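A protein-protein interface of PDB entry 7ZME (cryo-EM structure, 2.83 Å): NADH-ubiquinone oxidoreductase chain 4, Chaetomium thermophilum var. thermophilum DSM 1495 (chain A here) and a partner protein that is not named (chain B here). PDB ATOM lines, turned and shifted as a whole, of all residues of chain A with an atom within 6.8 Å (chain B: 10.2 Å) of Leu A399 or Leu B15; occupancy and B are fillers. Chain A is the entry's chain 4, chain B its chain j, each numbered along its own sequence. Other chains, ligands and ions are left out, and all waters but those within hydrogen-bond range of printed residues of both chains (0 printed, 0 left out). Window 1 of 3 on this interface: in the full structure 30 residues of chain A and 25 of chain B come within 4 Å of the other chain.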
ATOM      1  N   VAL A 337     -13.933  20.536   8.144  1.00  0.00           N
ATOM      2  CA  VAL A 337     -14.436  20.697   6.786  1.00  0.00           C
ATOM      3  C   VAL A 337     -13.334  20.596   5.741  1.00  0.00           C
ATOM      4  O   VAL A 337     -13.641  20.432   4.551  1.00  0.00           O
ATOM      5  CB  VAL A 337     -15.193  22.033   6.638  1.00  0.00           C
ATOM      6  CG1 VAL A 337     -16.393  22.053   7.564  1.00  0.00           C
ATOM      7  CG2 VAL A 337     -14.274  23.205   6.925  1.00  0.00           C
ATOM      8  N   ASP A 338     -12.073  20.704   6.137  1.00  0.00           N
ATOM      9  CA  ASP A 338     -10.969  20.368   5.253  1.00  0.00           C
ATOM     10  C   ASP A 338     -10.808  18.855   5.237  1.00  0.00           C
ATOM     11  O   ASP A 338     -10.695  18.224   6.292  1.00  0.00           O
ATOM     12  CB  ASP A 338      -9.689  21.056   5.724  1.00  0.00           C
ATOM     13  CG  ASP A 338      -8.483  20.749   4.847  1.00  0.00           C
ATOM     14  OD1 ASP A 338      -8.543  19.839   3.997  1.00  0.00           O
ATOM     15  OD2 ASP A 338      -7.455  21.434   5.014  1.00  0.00           O
ATOM     16  N   VAL A 339     -10.816  18.272   4.037  1.00  0.00           N
ATOM     17  CA  VAL A 339     -10.710  16.822   3.922  1.00  0.00           C
ATOM     18  C   VAL A 339      -9.325  16.355   4.344  1.00  0.00           C
ATOM     19  O   VAL A 339      -9.177  15.316   4.998  1.00  0.00           O
ATOM     20  CB  VAL A 339     -11.051  16.369   2.492  1.00  0.00           C
ATOM     21  CG1 VAL A 339     -11.123  14.856   2.421  1.00  0.00           C
ATOM     22  CG2 VAL A 339     -12.354  16.987   2.047  1.00  0.00           C
ATOM     23  N   THR A 395      -9.275  19.422  -8.142  1.00  0.00           N
ATOM     24  CA  THR A 395     -10.168  20.527  -7.822  1.00  0.00           C
ATOM     25  C   THR A 395      -9.466  21.780  -7.331  1.00  0.00           C
ATOM     26  O   THR A 395     -10.060  22.859  -7.393  1.00  0.00           O
ATOM     27  CB  THR A 395     -11.191  20.103  -6.756  1.00  0.00           C
ATOM     28  OG1 THR A 395     -10.512  19.787  -5.537  1.00  0.00           O
ATOM     29  CG2 THR A 395     -11.974  18.900  -7.213  1.00  0.00           C
ATOM     30  N   THR A 397      -9.065  22.528  -4.343  1.00  0.00           N
ATOM     31  CA  THR A 397      -9.681  22.894  -3.079  1.00  0.00           C
ATOM     32  C   THR A 397      -9.761  21.673  -2.176  1.00  0.00           C
ATOM     33  O   THR A 397      -9.894  20.541  -2.643  1.00  0.00           O
ATOM     34  CB  THR A 397     -11.084  23.502  -3.288  1.00  0.00           C
ATOM     35  OG1 THR A 397     -11.633  23.907  -2.028  1.00  0.00           O
ATOM     36  CG2 THR A 397     -12.019  22.507  -3.950  1.00  0.00           C
ATOM     37  N   ARG A 398      -9.654  21.916  -0.871  1.00  0.00           N
ATOM     38  CA  ARG A 398      -9.723  20.865   0.132  1.00  0.00           C
ATOM     39  C   ARG A 398     -11.028  20.891   0.912  1.00  0.00           C
ATOM     40  O   ARG A 398     -11.174  20.143   1.880  1.00  0.00           O
ATOM     41  CB  ARG A 398      -8.542  20.977   1.099  1.00  0.00           C
ATOM     42  CG  ARG A 398      -7.190  20.718   0.474  1.00  0.00           C
ATOM     43  CD  ARG A 398      -6.102  20.606   1.525  1.00  0.00           C
ATOM     44  NE  ARG A 398      -4.785  20.916   0.979  1.00  0.00           N
ATOM     45  CZ  ARG A 398      -4.077  20.095   0.209  1.00  0.00           C
ATOM     46  NH1 ARG A 398      -4.554  18.900  -0.115  1.00  0.00           N
ATOM     47  NH2 ARG A 398      -2.889  20.471  -0.242  1.00  0.00           N
ATOM     48  N   LEU A 399     -11.978  21.728   0.511  1.00  0.00           N
ATOM     49  CA  LEU A 399     -13.222  21.893   1.252  1.00  0.00           C
ATOM     50  C   LEU A 399     -14.189  20.777   0.888  1.00  0.00           C
ATOM     51  O   LEU A 399     -14.503  20.581  -0.289  1.00  0.00           O
ATOM     52  CB  LEU A 399     -13.838  23.256   0.951  1.00  0.00           C
ATOM     53  CG  LEU A 399     -13.080  24.480   1.456  1.00  0.00           C
ATOM     54  CD1 LEU A 399     -13.904  25.734   1.242  1.00  0.00           C
ATOM     55  CD2 LEU A 399     -12.722  24.315   2.918  1.00  0.00           C
ATOM     56  N   ILE A 400     -14.672  20.053   1.901  1.00  0.00           N
ATOM     57  CA  ILE A 400     -15.599  18.956   1.660  1.00  0.00           C
ATOM     58  C   ILE A 400     -16.936  19.459   1.129  1.00  0.00           C
ATOM     59  O   ILE A 400     -17.714  18.675   0.577  1.00  0.00           O
ATOM     60  CB  ILE A 400     -15.787  18.121   2.942  1.00  0.00           C
ATOM     61  CG1 ILE A 400     -16.314  16.724   2.600  1.00  0.00           C
ATOM     62  CG2 ILE A 400     -16.716  18.829   3.911  1.00  0.00           C
ATOM     63  CD1 ILE A 400     -16.096  15.695   3.679  1.00  0.00           C
ATOM     64  N   TYR A 401     -17.218  20.753   1.276  1.00  0.00           N
ATOM     65  CA  TYR A 401     -18.435  21.345   0.739  1.00  0.00           C
ATOM     66  C   TYR A 401     -18.576  21.149  -0.763  1.00  0.00           C
ATOM     67  O   TYR A 401     -19.694  20.948  -1.246  1.00  0.00           O
ATOM     68  CB  TYR A 401     -18.474  22.843   1.029  1.00  0.00           C
ATOM     69  CG  TYR A 401     -18.415  23.230   2.482  1.00  0.00           C
ATOM     70  CD1 TYR A 401     -19.124  22.524   3.440  1.00  0.00           C
ATOM     71  CD2 TYR A 401     -17.668  24.327   2.891  1.00  0.00           C
ATOM     72  CE1 TYR A 401     -19.080  22.891   4.769  1.00  0.00           C
ATOM     73  CE2 TYR A 401     -17.617  24.699   4.214  1.00  0.00           C
ATOM     74  CZ  TYR A 401     -18.325  23.978   5.149  1.00  0.00           C
ATOM     75  OH  TYR A 401     -18.277  24.351   6.471  1.00  0.00           O
ATOM     76  N   PHE A 402     -17.477  21.218  -1.505  1.00  0.00           N
ATOM     77  CA  PHE A 402     -17.502  21.160  -2.957  1.00  0.00           C
ATOM     78  C   PHE A 402     -17.570  19.743  -3.510  1.00  0.00           C
ATOM     79  O   PHE A 402     -17.752  19.583  -4.717  1.00  0.00           O
ATOM     80  CB  PHE A 402     -16.269  21.860  -3.530  1.00  0.00           C
ATOM     81  CG  PHE A 402     -16.241  23.338  -3.292  1.00  0.00           C
ATOM     82  CD1 PHE A 402     -16.961  24.193  -4.100  1.00  0.00           C
ATOM     83  CD2 PHE A 402     -15.483  23.872  -2.268  1.00  0.00           C
ATOM     84  CE1 PHE A 402     -16.934  25.552  -3.885  1.00  0.00           C
ATOM     85  CE2 PHE A 402     -15.452  25.232  -2.049  1.00  0.00           C
ATOM     86  CZ  PHE A 402     -16.179  26.074  -2.859  1.00  0.00           C
ATOM     87  N   PHE A 403     -17.425  18.718  -2.677  1.00  0.00           N
ATOM     88  CA  PHE A 403     -17.397  17.340  -3.141  1.00  0.00           C
ATOM     89  C   PHE A 403     -18.690  16.623  -2.786  1.00  0.00           C
ATOM     90  O   PHE A 403     -19.257  16.822  -1.708  1.00  0.00           O
ATOM     91  CB  PHE A 403     -16.220  16.566  -2.546  1.00  0.00           C
ATOM     92  CG  PHE A 403     -14.881  17.129  -2.901  1.00  0.00           C
ATOM     93  CD1 PHE A 403     -14.362  18.204  -2.211  1.00  0.00           C
ATOM     94  CD2 PHE A 403     -14.141  16.577  -3.926  1.00  0.00           C
ATOM     95  CE1 PHE A 403     -13.136  18.718  -2.535  1.00  0.00           C
ATOM     96  CE2 PHE A 403     -12.912  17.089  -4.254  1.00  0.00           C
ATOM     97  CZ  PHE A 403     -12.407  18.162  -3.555  1.00  0.00           C
ATOM     98  N   TYR A 481     -20.776  21.870  -8.215  1.00  0.00           N
ATOM     99  CA  TYR A 481     -19.676  22.800  -8.403  1.00  0.00           C
ATOM    100  C   TYR A 481     -18.638  22.272  -9.384  1.00  0.00           C
ATOM    101  O   TYR A 481     -17.705  23.003  -9.731  1.00  0.00           O
ATOM    102  CB  TYR A 481     -19.015  23.109  -7.061  1.00  0.00           C
ATOM    103  CG  TYR A 481     -19.982  23.519  -5.976  1.00  0.00           C
ATOM    104  CD1 TYR A 481     -20.591  22.572  -5.168  1.00  0.00           C
ATOM    105  CD2 TYR A 481     -20.273  24.856  -5.749  1.00  0.00           C
ATOM    106  CE1 TYR A 481     -21.470  22.944  -4.174  1.00  0.00           C
ATOM    107  CE2 TYR A 481     -21.151  25.237  -4.756  1.00  0.00           C
ATOM    108  CZ  TYR A 481     -21.748  24.277  -3.973  1.00  0.00           C
ATOM    109  OH  TYR A 481     -22.623  24.649  -2.982  1.00  0.00           O
ATOM    110  N   ILE B   9     -13.699  24.540 -11.579  1.00  0.00           N
ATOM    111  CA  ILE B   9     -14.576  24.358 -10.430  1.00  0.00           C
ATOM    112  C   ILE B   9     -15.433  25.605 -10.283  1.00  0.00           C
ATOM    113  O   ILE B   9     -14.915  26.726 -10.326  1.00  0.00           O
ATOM    114  CB  ILE B   9     -13.769  24.093  -9.145  1.00  0.00           C
ATOM    115  CG1 ILE B   9     -12.941  22.815  -9.287  1.00  0.00           C
ATOM    116  CG2 ILE B   9     -14.686  24.016  -7.923  1.00  0.00           C
ATOM    117  CD1 ILE B   9     -13.765  21.570  -9.434  1.00  0.00           C
ATOM    118  N   ALA B  10     -16.740  25.408 -10.112  1.00  0.00           N
ATOM    119  CA  ALA B  10     -17.671  26.506  -9.852  1.00  0.00           C
ATOM    120  C   ALA B  10     -17.474  26.968  -8.413  1.00  0.00           C
ATOM    121  O   ALA B  10     -18.211  26.604  -7.495  1.00  0.00           O
ATOM    122  CB  ALA B  10     -19.107  26.066 -10.099  1.00  0.00           C
ATOM    123  N   MET B  11     -16.451  27.792  -8.215  1.00  0.00           N
ATOM    124  CA  MET B  11     -16.044  28.189  -6.874  1.00  0.00           C
ATOM    125  C   MET B  11     -17.104  29.097  -6.270  1.00  0.00           C
ATOM    126  O   MET B  11     -17.304  30.226  -6.728  1.00  0.00           O
ATOM    127  CB  MET B  11     -14.688  28.881  -6.922  1.00  0.00           C
ATOM    128  CG  MET B  11     -13.518  27.922  -6.902  1.00  0.00           C
ATOM    129  SD  MET B  11     -13.529  26.825  -5.473  1.00  0.00           S
ATOM    130  CE  MET B  11     -11.857  26.194  -5.540  1.00  0.00           C
ATOM    131  N   ASP B  12     -17.783  28.610  -5.248  1.00  0.00           N
ATOM    132  CA  ASP B  12     -18.838  29.377  -4.610  1.00  0.00           C
ATOM    133  C   ASP B  12     -18.232  30.473  -3.745  1.00  0.00           C
ATOM    134  O   ASP B  12     -17.471  30.168  -2.820  1.00  0.00           O
ATOM    135  CB  ASP B  12     -19.709  28.451  -3.771  1.00  0.00           C
ATOM    136  CG  ASP B  12     -21.035  29.072  -3.405  1.00  0.00           C
ATOM    137  OD1 ASP B  12     -21.123  30.312  -3.337  1.00  0.00           O
ATOM    138  OD2 ASP B  12     -22.002  28.313  -3.198  1.00  0.00           O
ATOM    139  N   PRO B  13     -18.539  31.747  -3.998  1.00  0.00           N
ATOM    140  CA  PRO B  13     -17.974  32.812  -3.152  1.00  0.00           C
ATOM    141  C   PRO B  13     -18.334  32.683  -1.681  1.00  0.00           C
ATOM    142  O   PRO B  13     -17.504  32.986  -0.817  1.00  0.00           O
ATOM    143  CB  PRO B  13     -18.558  34.090  -3.771  1.00  0.00           C
ATOM    144  CG  PRO B  13     -18.892  33.711  -5.174  1.00  0.00           C
ATOM    145  CD  PRO B  13     -19.325  32.285  -5.118  1.00  0.00           C
ATOM    146  N   ALA B  14     -19.558  32.254  -1.369  1.00  0.00           N
ATOM    147  CA  ALA B  14     -19.944  32.082   0.028  1.00  0.00           C
ATOM    148  C   ALA B  14     -19.156  30.956   0.685  1.00  0.00           C
ATOM    149  O   ALA B  14     -18.711  31.086   1.830  1.00  0.00           O
ATOM    150  CB  ALA B  14     -21.443  31.817   0.129  1.00  0.00           C
ATOM    151  N   LEU B  15     -18.981  29.842  -0.027  1.00  0.00           N
ATOM    152  CA  LEU B  15     -18.254  28.706   0.524  1.00  0.00           C
ATOM    153  C   LEU B  15     -16.770  28.996   0.683  1.00  0.00           C
ATOM    154  O   LEU B  15     -16.143  28.496   1.620  1.00  0.00           O
ATOM    155  CB  LEU B  15     -18.465  27.478  -0.358  1.00  0.00           C
ATOM    156  CG  LEU B  15     -19.677  26.592  -0.079  1.00  0.00           C
ATOM    157  CD1 LEU B  15     -20.968  27.324  -0.288  1.00  0.00           C
ATOM    158  CD2 LEU B  15     -19.614  25.418  -1.021  1.00  0.00           C
ATOM    159  N   VAL B  16     -16.188  29.793  -0.215  1.00  0.00           N
ATOM    160  CA  VAL B  16     -14.770  30.101  -0.087  1.00  0.00           C
ATOM    161  C   VAL B  16     -14.509  31.155   0.979  1.00  0.00           C
ATOM    162  O   VAL B  16     -13.385  31.245   1.484  1.00  0.00           O
ATOM    163  CB  VAL B  16     -14.175  30.546  -1.432  1.00  0.00           C
ATOM    164  CG1 VAL B  16     -14.416  29.484  -2.490  1.00  0.00           C
ATOM    165  CG2 VAL B  16     -14.745  31.881  -1.856  1.00  0.00           C
ATOM    166  N   ARG B  17     -15.513  31.948   1.346  1.00  0.00           N
ATOM    167  CA  ARG B  17     -15.339  32.893   2.438  1.00  0.00           C
ATOM    168  C   ARG B  17     -15.635  32.259   3.785  1.00  0.00           C
ATOM    169  O   ARG B  17     -15.081  32.695   4.799  1.00  0.00           O
ATOM    170  CB  ARG B  17     -16.216  34.131   2.220  1.00  0.00           C
ATOM    171  CG  ARG B  17     -17.493  34.178   3.038  1.00  0.00           C
ATOM    172  CD  ARG B  17     -18.318  35.401   2.690  1.00  0.00           C
ATOM    173  NE  ARG B  17     -18.740  35.388   1.293  1.00  0.00           N
ATOM    174  CZ  ARG B  17     -19.280  36.428   0.667  1.00  0.00           C
ATOM    175  NH1 ARG B  17     -19.633  36.326  -0.608  1.00  0.00           N
ATOM    176  NH2 ARG B  17     -19.468  37.570   1.313  1.00  0.00           N
ATOM    177  N   LEU B  18     -16.487  31.234   3.816  1.00  0.00           N
ATOM    178  CA  LEU B  18     -16.632  30.430   5.023  1.00  0.00           C
ATOM    179  C   LEU B  18     -15.336  29.698   5.349  1.00  0.00           C
ATOM    180  O   LEU B  18     -14.908  29.662   6.507  1.00  0.00           O
ATOM    181  CB  LEU B  18     -17.781  29.438   4.855  1.00  0.00           C
ATOM    182  CG  LEU B  18     -18.135  28.575   6.067  1.00  0.00           C
ATOM    183  CD1 LEU B  18     -18.306  29.425   7.304  1.00  0.00           C
ATOM    184  CD2 LEU B  18     -19.388  27.777   5.795  1.00  0.00           C
ATOM    185  N   GLY B  19     -14.697  29.113   4.335  1.00  0.00           N
ATOM    186  CA  GLY B  19     -13.437  28.425   4.563  1.00  0.00           C
ATOM    187  C   GLY B  19     -12.327  29.360   4.998  1.00  0.00           C
ATOM    188  O   GLY B  19     -11.473  28.987   5.807  1.00  0.00           O
ATOM    189  N   SER B  20     -12.314  30.583   4.465  1.00  0.00           N
ATOM    190  CA  SER B  20     -11.319  31.561   4.892  1.00  0.00           C
ATOM    191  C   SER B  20     -11.574  32.016   6.321  1.00  0.00           C
ATOM    192  O   SER B  20     -10.628  32.221   7.087  1.00  0.00           O
ATOM    193  CB  SER B  20     -11.311  32.755   3.940  1.00  0.00           C
ATOM    194  OG  SER B  20     -12.401  33.620   4.199  1.00  0.00           O
ATOM    195  N   MET B  21     -12.843  32.182   6.697  1.00  0.00           N
ATOM    196  CA  MET B  21     -13.169  32.545   8.072  1.00  0.00           C
ATOM    197  C   MET B  21     -12.769  31.443   9.042  1.00  0.00           C
ATOM    198  O   MET B  21     -12.196  31.717  10.102  1.00  0.00           O
ATOM    199  CB  MET B  21     -14.663  32.858   8.186  1.00  0.00           C
ATOM    200  CG  MET B  21     -15.126  33.312   9.565  1.00  0.00           C
ATOM    201  SD  MET B  21     -15.438  31.977  10.740  1.00  0.00           S
ATOM    202  CE  MET B  21     -16.950  31.293  10.080  1.00  0.00           C
ATOM    203  N   ILE B  22     -13.075  30.192   8.702  1.00  0.00           N
ATOM    204  CA  ILE B  22     -12.714  29.072   9.563  1.00  0.00           C
ATOM    205  C   ILE B  22     -11.200  28.958   9.674  1.00  0.00           C
ATOM    206  O   ILE B  22     -10.659  28.678  10.749  1.00  0.00           O
ATOM    207  CB  ILE B  22     -13.350  27.776   9.030  1.00  0.00           C
ATOM    208  CG1 ILE B  22     -14.864  27.809   9.233  1.00  0.00           C
ATOM    209  CG2 ILE B  22     -12.754  26.555   9.710  1.00  0.00           C
ATOM    210  CD1 ILE B  22     -15.610  26.795   8.402  1.00  0.00           C
ATOM    211  N   SER B  23     -10.494  29.189   8.566  1.00  0.00           N
ATOM    212  CA  SER B  23      -9.036  29.139   8.581  1.00  0.00           C
ATOM    213  C   SER B  23      -8.446  30.241   9.448  1.00  0.00           C
ATOM    214  O   SER B  23      -7.435  30.032  10.126  1.00  0.00           O
ATOM    215  CB  SER B  23      -8.495  29.243   7.157  1.00  0.00           C
ATOM    216  OG  SER B  23      -7.080  29.229   7.154  1.00  0.00           O
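The backbone carbonyl oxygen of Tyr A481 sits at hydrogen-bond distance from the backbone NH of Ala B10, 2.6 Å away.
OD1 of Asp B12 sits at hydrogen-bond distance from N of Ala B14 (3.2 Å).
OG1 of Thr A395 lies within hydrogen-bond range of O of Thr A397 (3.1 Å).
The side-chain hydroxyl (OG1) of Thr A397 is in hydrogen-bond range of the backbone NH (N) of Leu A399 (3.4 Å).
Ile B9 touches Thr A395 (CG1 to O, 3.4 Å).
CB of Thr A397 touches CE of Met B11, at 3.6 Å.
Tyr A401 touches Leu B15 (CB to CD2, 3.5 Å).
O of Ala B10 touches CE1 of Phe A402 (3.97 Å).
Phe A402 touches Asp B12.
Leu B15 touches Phe A402 (CB to CZ, 3.7 Å).
Val B16 touches Phe A402 (CG1 to CZ, 3.9 Å).
O of Tyr A481 touches CA of Ile B9, at 3.5 Å.
Asp B12 touches Tyr A481.
Leu B15 touches Tyr A481 (CD2 to OH, 3.7 Å).
Leu A399 touches just one residue of chain B: Leu B15.
Leu B15 touches just these residues of chain A: Leu A399 (3.6 Å), Tyr A401 (3.5 Å), Phe A402 (3.7 Å) and Tyr A481 (3.7 Å).
Thr A397 touches one residue of chain B.
No residue of chain B comes within 4 Å of Ile A400.
Phe A402 touches just these residues of chain B: Ala B10 (3.97 Å), Met B11 (3.8 Å), Asp B12 (3.5 Å), Leu B15 (3.7 Å) and Val B16 (3.9 Å).
Printed residues of chain B within 4 Å of Tyr A481: Ile B9 (3.5 Å), Ala B10 (2.6 Å), Asp B12 (3.6 Å) and Leu B15 (3.7 Å).
Printed residues of chain A within 4 Å of Leu B18: Tyr A401 (3.7 Å).
Printed residues of chain B within 4 Å of Tyr A401: Leu B15 (3.5 Å) and Leu B18 (3.7 Å).
Ala B14 touches none of the printed residues of chain A.
Met B21 touches none of the printed residues of chain A.
The nearest printed residue of chain A that does not touch Leu B15 is Ile A400 (6.9 Å).
The nearest printed residue of chain A that does not touch Met B11 is Thr A395 (4.2 Å).
Of the 15 printed residues of chain B, 7 touch a printed residue of chain A.
Along chain B the printed residues that touch a printed residue of chain A span positions 9 to 18.
Of the 12 printed residues of chain A, 6 touch a printed residue of chain B.
Hydrophobic or aromatic side chains of chain A within 4 Å of the printed part of chain B: Leu A399, Tyr A401, Phe A402 and Tyr A481.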
